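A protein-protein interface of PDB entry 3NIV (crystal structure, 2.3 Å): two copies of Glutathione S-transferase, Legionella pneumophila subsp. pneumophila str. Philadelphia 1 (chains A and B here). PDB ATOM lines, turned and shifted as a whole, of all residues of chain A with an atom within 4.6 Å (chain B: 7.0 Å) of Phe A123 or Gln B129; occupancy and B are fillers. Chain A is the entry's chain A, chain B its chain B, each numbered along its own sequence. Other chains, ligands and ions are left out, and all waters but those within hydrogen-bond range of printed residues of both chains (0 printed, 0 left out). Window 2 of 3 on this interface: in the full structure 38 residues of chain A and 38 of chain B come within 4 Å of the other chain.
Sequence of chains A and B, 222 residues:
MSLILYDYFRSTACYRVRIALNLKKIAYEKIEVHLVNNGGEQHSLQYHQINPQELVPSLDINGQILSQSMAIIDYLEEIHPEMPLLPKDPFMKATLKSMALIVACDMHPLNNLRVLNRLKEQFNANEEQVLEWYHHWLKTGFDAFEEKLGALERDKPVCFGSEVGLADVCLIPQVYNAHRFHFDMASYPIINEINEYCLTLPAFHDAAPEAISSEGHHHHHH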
ATOM      1  N   ARG A 118      19.226 -26.209  17.284  1.00  0.00           N
ATOM      2  CA  ARG A 118      18.503 -26.615  16.094  1.00  0.00           C
ATOM      3  C   ARG A 118      19.407 -27.439  15.180  1.00  0.00           C
ATOM      4  O   ARG A 118      18.952 -28.371  14.522  1.00  0.00           O
ATOM      5  CB  ARG A 118      17.966 -25.401  15.340  1.00  0.00           C
ATOM      6  CG  ARG A 118      17.091 -25.770  14.155  1.00  0.00           C
ATOM      7  CD  ARG A 118      15.648 -26.036  14.571  1.00  0.00           C
ATOM      8  NE  ARG A 118      14.856 -26.486  13.432  1.00  0.00           N
ATOM      9  CZ  ARG A 118      13.611 -26.940  13.510  1.00  0.00           C
ATOM     10  NH1 ARG A 118      12.990 -27.004  14.677  1.00  0.00           N
ATOM     11  NH2 ARG A 118      12.990 -27.333  12.411  1.00  0.00           N
ATOM     12  N   LEU A 119      20.686 -27.084  15.126  1.00  0.00           N
ATOM     13  CA  LEU A 119      21.628 -27.835  14.306  1.00  0.00           C
ATOM     14  C   LEU A 119      21.766 -29.238  14.857  1.00  0.00           C
ATOM     15  O   LEU A 119      21.852 -30.205  14.112  1.00  0.00           O
ATOM     16  CB  LEU A 119      22.992 -27.161  14.294  1.00  0.00           C
ATOM     17  CG  LEU A 119      22.960 -25.805  13.601  1.00  0.00           C
ATOM     18  CD1 LEU A 119      24.348 -25.203  13.625  1.00  0.00           C
ATOM     19  CD2 LEU A 119      22.440 -25.954  12.174  1.00  0.00           C
ATOM     20  N   LYS A 120      21.771 -29.334  16.180  1.00  0.00           N
ATOM     21  CA  LYS A 120      21.872 -30.618  16.853  1.00  0.00           C
ATOM     22  C   LYS A 120      20.587 -31.440  16.707  1.00  0.00           C
ATOM     23  O   LYS A 120      20.643 -32.632  16.427  1.00  0.00           O
ATOM     24  CB  LYS A 120      22.264 -30.418  18.317  1.00  0.00           C
ATOM     25  CG  LYS A 120      23.756 -30.281  18.489  1.00  0.00           C
ATOM     26  CD  LYS A 120      24.148 -29.231  19.505  1.00  0.00           C
ATOM     27  CE  LYS A 120      24.121 -29.765  20.921  1.00  0.00           C
ATOM     28  NZ  LYS A 120      24.829 -28.816  21.829  1.00  0.00           N
ATOM     29  N   GLU A 121      19.435 -30.809  16.883  1.00  0.00           N
ATOM     30  CA  GLU A 121      18.180 -31.508  16.696  1.00  0.00           C
ATOM     31  C   GLU A 121      18.046 -31.963  15.238  1.00  0.00           C
ATOM     32  O   GLU A 121      18.099 -33.154  14.939  1.00  0.00           O
ATOM     33  CB  GLU A 121      17.003 -30.611  17.077  1.00  0.00           C
ATOM     34  CG  GLU A 121      15.634 -31.206  16.726  1.00  0.00           C
ATOM     35  CD  GLU A 121      14.664 -30.154  16.192  1.00  0.00           C
ATOM     36  OE1 GLU A 121      14.628 -29.035  16.766  1.00  0.00           O
ATOM     37  OE2 GLU A 121      13.937 -30.445  15.199  1.00  0.00           O
ATOM     38  N   GLN A 122      17.890 -31.006  14.332  1.00  0.00           N
ATOM     39  CA  GLN A 122      17.636 -31.306  12.931  1.00  0.00           C
ATOM     40  C   GLN A 122      18.722 -32.128  12.282  1.00  0.00           C
ATOM     41  O   GLN A 122      18.447 -32.967  11.425  1.00  0.00           O
ATOM     42  CB  GLN A 122      17.494 -30.019  12.123  1.00  0.00           C
ATOM     43  CG  GLN A 122      16.088 -29.499  12.025  1.00  0.00           C
ATOM     44  CD  GLN A 122      15.922 -28.527  10.871  1.00  0.00           C
ATOM     45  OE1 GLN A 122      15.647 -27.348  11.078  1.00  0.00           O
ATOM     46  NE2 GLN A 122      16.087 -29.022   9.646  1.00  0.00           N
ATOM     47  N   PHE A 123      19.965 -31.858  12.647  1.00  0.00           N
ATOM     48  CA  PHE A 123      21.069 -32.396  11.871  1.00  0.00           C
ATOM     49  C   PHE A 123      22.031 -33.213  12.721  1.00  0.00           C
ATOM     50  O   PHE A 123      23.044 -33.702  12.226  1.00  0.00           O
ATOM     51  CB  PHE A 123      21.805 -31.268  11.139  1.00  0.00           C
ATOM     52  CG  PHE A 123      20.928 -30.461  10.234  1.00  0.00           C
ATOM     53  CD1 PHE A 123      20.552 -30.951   8.991  1.00  0.00           C
ATOM     54  CD2 PHE A 123      20.477 -29.206  10.622  1.00  0.00           C
ATOM     55  CE1 PHE A 123      19.740 -30.204   8.145  1.00  0.00           C
ATOM     56  CE2 PHE A 123      19.661 -28.448   9.779  1.00  0.00           C
ATOM     57  CZ  PHE A 123      19.292 -28.950   8.542  1.00  0.00           C
ATOM     58  N   ASN A 124      21.696 -33.375  13.995  1.00  0.00           N
ATOM     59  CA  ASN A 124      22.563 -34.086  14.915  1.00  0.00           C
ATOM     60  C   ASN A 124      23.993 -33.636  14.724  1.00  0.00           C
ATOM     61  O   ASN A 124      24.898 -34.463  14.633  1.00  0.00           O
ATOM     62  CB  ASN A 124      22.471 -35.600  14.700  1.00  0.00           C
ATOM     63  CG  ASN A 124      21.056 -36.136  14.868  1.00  0.00           C
ATOM     64  OD1 ASN A 124      20.426 -35.979  15.924  1.00  0.00           O
ATOM     65  ND2 ASN A 124      20.551 -36.783  13.823  1.00  0.00           N
ATOM     66  N   ALA A 125      24.194 -32.326  14.633  1.00  0.00           N
ATOM     67  CA  ALA A 125      25.537 -31.766  14.522  1.00  0.00           C
ATOM     68  C   ALA A 125      26.455 -32.224  15.670  1.00  0.00           C
ATOM     69  O   ALA A 125      26.131 -32.056  16.850  1.00  0.00           O
ATOM     70  CB  ALA A 125      25.475 -30.243  14.463  1.00  0.00           C
ATOM     71  N   LEU B 119      23.614 -24.606   5.239  1.00  0.00           N
ATOM     72  CA  LEU B 119      22.958 -25.840   5.673  1.00  0.00           C
ATOM     73  C   LEU B 119      23.144 -26.950   4.651  1.00  0.00           C
ATOM     74  O   LEU B 119      23.387 -28.105   5.007  1.00  0.00           O
ATOM     75  CB  LEU B 119      21.470 -25.622   5.906  1.00  0.00           C
ATOM     76  CG  LEU B 119      21.091 -24.703   7.060  1.00  0.00           C
ATOM     77  CD1 LEU B 119      19.565 -24.486   7.130  1.00  0.00           C
ATOM     78  CD2 LEU B 119      21.641 -25.251   8.366  1.00  0.00           C
ATOM     79  N   LYS B 120      23.033 -26.600   3.377  1.00  0.00           N
ATOM     80  CA  LYS B 120      23.214 -27.590   2.325  1.00  0.00           C
ATOM     81  C   LYS B 120      24.692 -27.939   2.145  1.00  0.00           C
ATOM     82  O   LYS B 120      25.035 -29.055   1.784  1.00  0.00           O
ATOM     83  CB  LYS B 120      22.620 -27.073   1.011  1.00  0.00           C
ATOM     84  CG  LYS B 120      21.156 -26.679   1.127  1.00  0.00           C
ATOM     85  CD  LYS B 120      20.794 -25.481   0.259  1.00  0.00           C
ATOM     86  CE  LYS B 120      20.934 -25.778  -1.225  1.00  0.00           C
ATOM     87  NZ  LYS B 120      20.143 -24.831  -2.074  1.00  0.00           N
ATOM     88  N   PHE B 123      25.636 -29.550   5.977  1.00  0.00           N
ATOM     89  CA  PHE B 123      24.801 -30.643   6.446  1.00  0.00           C
ATOM     90  C   PHE B 123      24.115 -31.343   5.289  1.00  0.00           C
ATOM     91  O   PHE B 123      23.238 -32.197   5.474  1.00  0.00           O
ATOM     92  CB  PHE B 123      23.788 -30.121   7.454  1.00  0.00           C
ATOM     93  CG  PHE B 123      24.420 -29.489   8.650  1.00  0.00           C
ATOM     94  CD1 PHE B 123      24.995 -30.277   9.644  1.00  0.00           C
ATOM     95  CD2 PHE B 123      24.463 -28.114   8.780  1.00  0.00           C
ATOM     96  CE1 PHE B 123      25.596 -29.697  10.750  1.00  0.00           C
ATOM     97  CE2 PHE B 123      25.049 -27.529   9.886  1.00  0.00           C
ATOM     98  CZ  PHE B 123      25.619 -28.317  10.872  1.00  0.00           C
ATOM     99  N   ASN B 124      24.542 -30.983   4.085  1.00  0.00           N
ATOM    100  CA  ASN B 124      23.894 -31.477   2.891  1.00  0.00           C
ATOM    101  C   ASN B 124      22.396 -31.602   3.127  1.00  0.00           C
ATOM    102  O   ASN B 124      21.811 -32.653   2.891  1.00  0.00           O
ATOM    103  CB  ASN B 124      24.478 -32.827   2.493  1.00  0.00           C
ATOM    104  CG  ASN B 124      24.179 -33.176   1.056  1.00  0.00           C
ATOM    105  OD1 ASN B 124      24.427 -32.377   0.146  1.00  0.00           O
ATOM    106  ND2 ASN B 124      23.634 -34.373   0.836  1.00  0.00           N
ATOM    107  N   ALA B 125      21.785 -30.528   3.620  1.00  0.00           N
ATOM    108  CA  ALA B 125      20.356 -30.530   3.912  1.00  0.00           C
ATOM    109  C   ALA B 125      19.580 -30.641   2.615  1.00  0.00           C
ATOM    110  O   ALA B 125      20.066 -30.228   1.566  1.00  0.00           O
ATOM    111  CB  ALA B 125      19.962 -29.269   4.663  1.00  0.00           C
ATOM    112  N   ASN B 126      18.381 -31.210   2.680  1.00  0.00           N
ATOM    113  CA  ASN B 126      17.534 -31.303   1.495  1.00  0.00           C
ATOM    114  C   ASN B 126      16.424 -30.260   1.515  1.00  0.00           C
ATOM    115  O   ASN B 126      16.240 -29.557   2.516  1.00  0.00           O
ATOM    116  CB  ASN B 126      16.942 -32.708   1.350  1.00  0.00           C
ATOM    117  CG  ASN B 126      16.232 -33.169   2.602  1.00  0.00           C
ATOM    118  OD1 ASN B 126      15.387 -32.459   3.148  1.00  0.00           O
ATOM    119  ND2 ASN B 126      16.573 -34.365   3.070  1.00  0.00           N
ATOM    120  N   GLU B 127      15.685 -30.172   0.413  1.00  0.00           N
ATOM    121  CA  GLU B 127      14.627 -29.184   0.291  1.00  0.00           C
ATOM    122  C   GLU B 127      13.784 -29.157   1.560  1.00  0.00           C
ATOM    123  O   GLU B 127      13.652 -28.118   2.199  1.00  0.00           O
ATOM    124  CB  GLU B 127      13.757 -29.460  -0.942  1.00  0.00           C
ATOM    125  CG  GLU B 127      13.081 -28.201  -1.520  1.00  0.00           C
ATOM    126  CD  GLU B 127      12.139 -28.490  -2.695  1.00  0.00           C
ATOM    127  OE1 GLU B 127      12.064 -29.659  -3.144  1.00  0.00           O
ATOM    128  OE2 GLU B 127      11.475 -27.540  -3.170  1.00  0.00           O
ATOM    129  N   GLU B 128      13.243 -30.307   1.942  1.00  0.00           N
ATOM    130  CA  GLU B 128      12.322 -30.388   3.078  1.00  0.00           C
ATOM    131  C   GLU B 128      12.969 -30.033   4.419  1.00  0.00           C
ATOM    132  O   GLU B 128      12.284 -29.636   5.360  1.00  0.00           O
ATOM    133  CB  GLU B 128      11.675 -31.781   3.136  1.00  0.00           C
ATOM    134  CG  GLU B 128      11.277 -32.259   4.530  1.00  0.00           C
ATOM    135  CD  GLU B 128      10.768 -33.694   4.520  1.00  0.00           C
ATOM    136  OE1 GLU B 128      10.191 -34.103   3.488  1.00  0.00           O
ATOM    137  OE2 GLU B 128      10.947 -34.413   5.533  1.00  0.00           O
ATOM    138  N   GLN B 129      14.285 -30.182   4.513  1.00  0.00           N
ATOM    139  CA  GLN B 129      14.986 -29.811   5.734  1.00  0.00           C
ATOM    140  C   GLN B 129      15.175 -28.293   5.790  1.00  0.00           C
ATOM    141  O   GLN B 129      15.003 -27.664   6.839  1.00  0.00           O
ATOM    142  CB  GLN B 129      16.334 -30.532   5.826  1.00  0.00           C
ATOM    143  CG  GLN B 129      16.212 -32.010   6.152  1.00  0.00           C
ATOM    144  CD  GLN B 129      17.555 -32.659   6.445  1.00  0.00           C
ATOM    145  OE1 GLN B 129      18.453 -32.674   5.600  1.00  0.00           O
ATOM    146  NE2 GLN B 129      17.692 -33.210   7.646  1.00  0.00           N
ATOM    147  N   VAL B 130      15.520 -27.711   4.648  1.00  0.00           N
ATOM    148  CA  VAL B 130      15.636 -26.269   4.551  1.00  0.00           C
ATOM    149  C   VAL B 130      14.302 -25.619   4.932  1.00  0.00           C
ATOM    150  O   VAL B 130      14.272 -24.650   5.684  1.00  0.00           O
ATOM    151  CB  VAL B 130      16.071 -25.845   3.145  1.00  0.00           C
ATOM    152  CG1 VAL B 130      16.352 -24.368   3.108  1.00  0.00           C
ATOM    153  CG2 VAL B 130      17.302 -26.615   2.736  1.00  0.00           C
ATOM    154  N   LEU B 131      13.201 -26.183   4.445  1.00  0.00           N
ATOM    155  CA  LEU B 131      11.868 -25.659   4.750  1.00  0.00           C
ATOM    156  C   LEU B 131      11.499 -25.735   6.222  1.00  0.00           C
ATOM    157  O   LEU B 131      10.884 -24.816   6.757  1.00  0.00           O
ATOM    158  CB  LEU B 131      10.795 -26.390   3.946  1.00  0.00           C
ATOM    159  CG  LEU B 131      10.113 -25.598   2.834  1.00  0.00           C
ATOM    160  CD1 LEU B 131       9.623 -24.272   3.381  1.00  0.00           C
ATOM    161  CD2 LEU B 131      11.077 -25.392   1.677  1.00  0.00           C
ATOM    162  N   GLU B 132      11.838 -26.845   6.866  1.00  0.00           N
ATOM    163  CA  GLU B 132      11.547 -27.019   8.286  1.00  0.00           C
ATOM    164  C   GLU B 132      12.260 -25.932   9.083  1.00  0.00           C
ATOM    165  O   GLU B 132      11.686 -25.338   9.998  1.00  0.00           O
ATOM    166  CB  GLU B 132      11.969 -28.418   8.758  1.00  0.00           C
ATOM    167  CG  GLU B 132      10.997 -29.527   8.351  1.00  0.00           C
ATOM    168  CD  GLU B 132      11.557 -30.954   8.524  1.00  0.00           C
ATOM    169  OE1 GLU B 132      12.603 -31.134   9.205  1.00  0.00           O
ATOM    170  OE2 GLU B 132      10.937 -31.896   7.968  1.00  0.00           O
ATOM    171  N   TRP B 133      13.510 -25.673   8.702  1.00  0.00           N
ATOM    172  CA  TRP B 133      14.335 -24.624   9.299  1.00  0.00           C
ATOM    173  C   TRP B 133      13.633 -23.292   9.105  1.00  0.00           C
ATOM    174  O   TRP B 133      13.224 -22.644  10.069  1.00  0.00           O
ATOM    175  CB  TRP B 133      15.706 -24.621   8.608  1.00  0.00           C
ATOM    176  CG  TRP B 133      16.675 -23.500   8.949  1.00  0.00           C
ATOM    177  CD1 TRP B 133      16.768 -22.274   8.339  1.00  0.00           C
ATOM    178  CD2 TRP B 133      17.737 -23.543   9.923  1.00  0.00           C
ATOM    179  NE1 TRP B 133      17.800 -21.549   8.895  1.00  0.00           N
ATOM    180  CE2 TRP B 133      18.405 -22.302   9.868  1.00  0.00           C
ATOM    181  CE3 TRP B 133      18.171 -24.504  10.847  1.00  0.00           C
ATOM    182  CZ2 TRP B 133      19.492 -21.996  10.708  1.00  0.00           C
ATOM    183  CZ3 TRP B 133      19.258 -24.202  11.678  1.00  0.00           C
ATOM    184  CH2 TRP B 133      19.901 -22.958  11.604  1.00  0.00           C
ATOM    185  N   TYR B 134      13.469 -22.921   7.841  1.00  0.00           N
ATOM    186  CA  TYR B 134      12.875 -21.656   7.455  1.00  0.00           C
ATOM    187  C   TYR B 134      11.565 -21.362   8.198  1.00  0.00           C
ATOM    188  O   TYR B 134      11.351 -20.238   8.669  1.00  0.00           O
ATOM    189  CB  TYR B 134      12.652 -21.632   5.938  1.00  0.00           C
ATOM    190  CG  TYR B 134      12.547 -20.237   5.349  1.00  0.00           C
ATOM    191  CD1 TYR B 134      11.464 -19.417   5.628  1.00  0.00           C
ATOM    192  CD2 TYR B 134      13.539 -19.742   4.513  1.00  0.00           C
ATOM    193  CE1 TYR B 134      11.372 -18.135   5.099  1.00  0.00           C
ATOM    194  CE2 TYR B 134      13.457 -18.465   3.978  1.00  0.00           C
ATOM    195  CZ  TYR B 134      12.369 -17.666   4.273  1.00  0.00           C
ATOM    196  OH  TYR B 134      12.298 -16.401   3.735  1.00  0.00           O
ATOM    197  N   HIS B 135      10.700 -22.371   8.292  1.00  0.00           N
ATOM    198  CA  HIS B 135       9.384 -22.233   8.922  1.00  0.00           C
ATOM    199  C   HIS B 135       9.463 -22.109  10.436  1.00  0.00           C
ATOM    200  O   HIS B 135       8.621 -21.451  11.058  1.00  0.00           O
ATOM    201  CB  HIS B 135       8.510 -23.436   8.573  1.00  0.00           C
ATOM    202  CG  HIS B 135       7.929 -23.375   7.200  1.00  0.00           C
ATOM    203  ND1 HIS B 135       6.860 -24.156   6.807  1.00  0.00           N
ATOM    204  CD2 HIS B 135       8.244 -22.601   6.135  1.00  0.00           C
ATOM    205  CE1 HIS B 135       6.559 -23.880   5.553  1.00  0.00           C
ATOM    206  NE2 HIS B 135       7.376 -22.936   5.122  1.00  0.00           N
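NH2 of Arg A118 sits at hydrogen-bond distance from O of Glu B132, 3.4 Å away. The side-chain amide nitrogen (NE2) of Gln A122 lies within hydrogen-bond range of the backbone carbonyl oxygen (O) of Gln B129, at 3.3 Å.
The side-chain carboxylate (OE1) of Glu A121 lies within salt-bridge range of the guanidinium group (NH1) of Arg A118, at 3.3 Å. NE of Arg A118 is in hydrogen-bond range of OE1 of Gln A122 (2.6 Å). N of Asn A124 sits at hydrogen-bond distance from O of Leu A119 (3.2 Å). The backbone carbonyl oxygen of Leu B119 sits at hydrogen-bond distance from the backbone NH of Asn B124 (3.2 Å). The backbone carbonyl oxygen (O) of Leu B119 sits at hydrogen-bond distance from the backbone NH (N) of Ala B125 (3.2 Å). OD1 of Asn B126 sits at hydrogen-bond distance from N of Gln B129, 2.9 Å away.
Among the printed residues, merely in contact across the chains: Gln A122 with Trp B133 (3.5 Å), Phe A123 with Ala B125 (3.6 Å), Arg A118 with Trp B133 (3.6 Å), Phe A123 with Phe B123 (3.7 Å), Leu A119 with Trp B133 (3.7 Å), Phe A123 with Gln B129 (3.7 Å), Ala A125 with Phe B123 (3.8 Å), Leu A119 with Phe B123 (3.8 Å) and Leu A119 with Leu B119 (3.95 Å).
Of the printed residues of chain B, Phe A123 touches Phe B123 (3.7 Å), Ala B125 (3.6 Å) and Gln B129 (3.7 Å). Asn A124 touches none of the printed residues of chain B. Printed residues of chain B within 4 Å of Ala A125: Phe B123 (3.8 Å). Of the printed residues of chain A, Leu B119 touches Leu A119. The nearest printed residue of chain B that does not touch Phe A123 is Leu B119 (4.02 Å). The nearest printed residue of chain B that does not touch Leu A119 is Gln B129 (8.3 Å).
Hydrophobic or aromatic side chains of chain B within 4 Å of the printed part of chain A: Leu B119, Phe B123, Ala B125 and Trp B133. Of the 8 printed residues of chain A, 5 touch a printed residue of chain B. Hydrophobic or aromatic side chains of chain A within 4 Å of the printed part of chain B: Leu A119, Phe A123 and Ala A125.
Leu B119 touches its own counterpart, Leu A119. Leu A119 touches Phe B123, but with the chains exchanged Phe A123 does not touch Leu B119 (4.02 Å). Phe B123 touches its own counterpart, Phe A123. Phe A123 touches Ala B125, and with the chains exchanged Ala A125 touches Phe B123. Positions printed for both chains: 119, 120, 123, 124 and 125. Of the 11 pairs that touch across the chains among the printed residues, 4 have their exchanged pair printed and touching as well.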
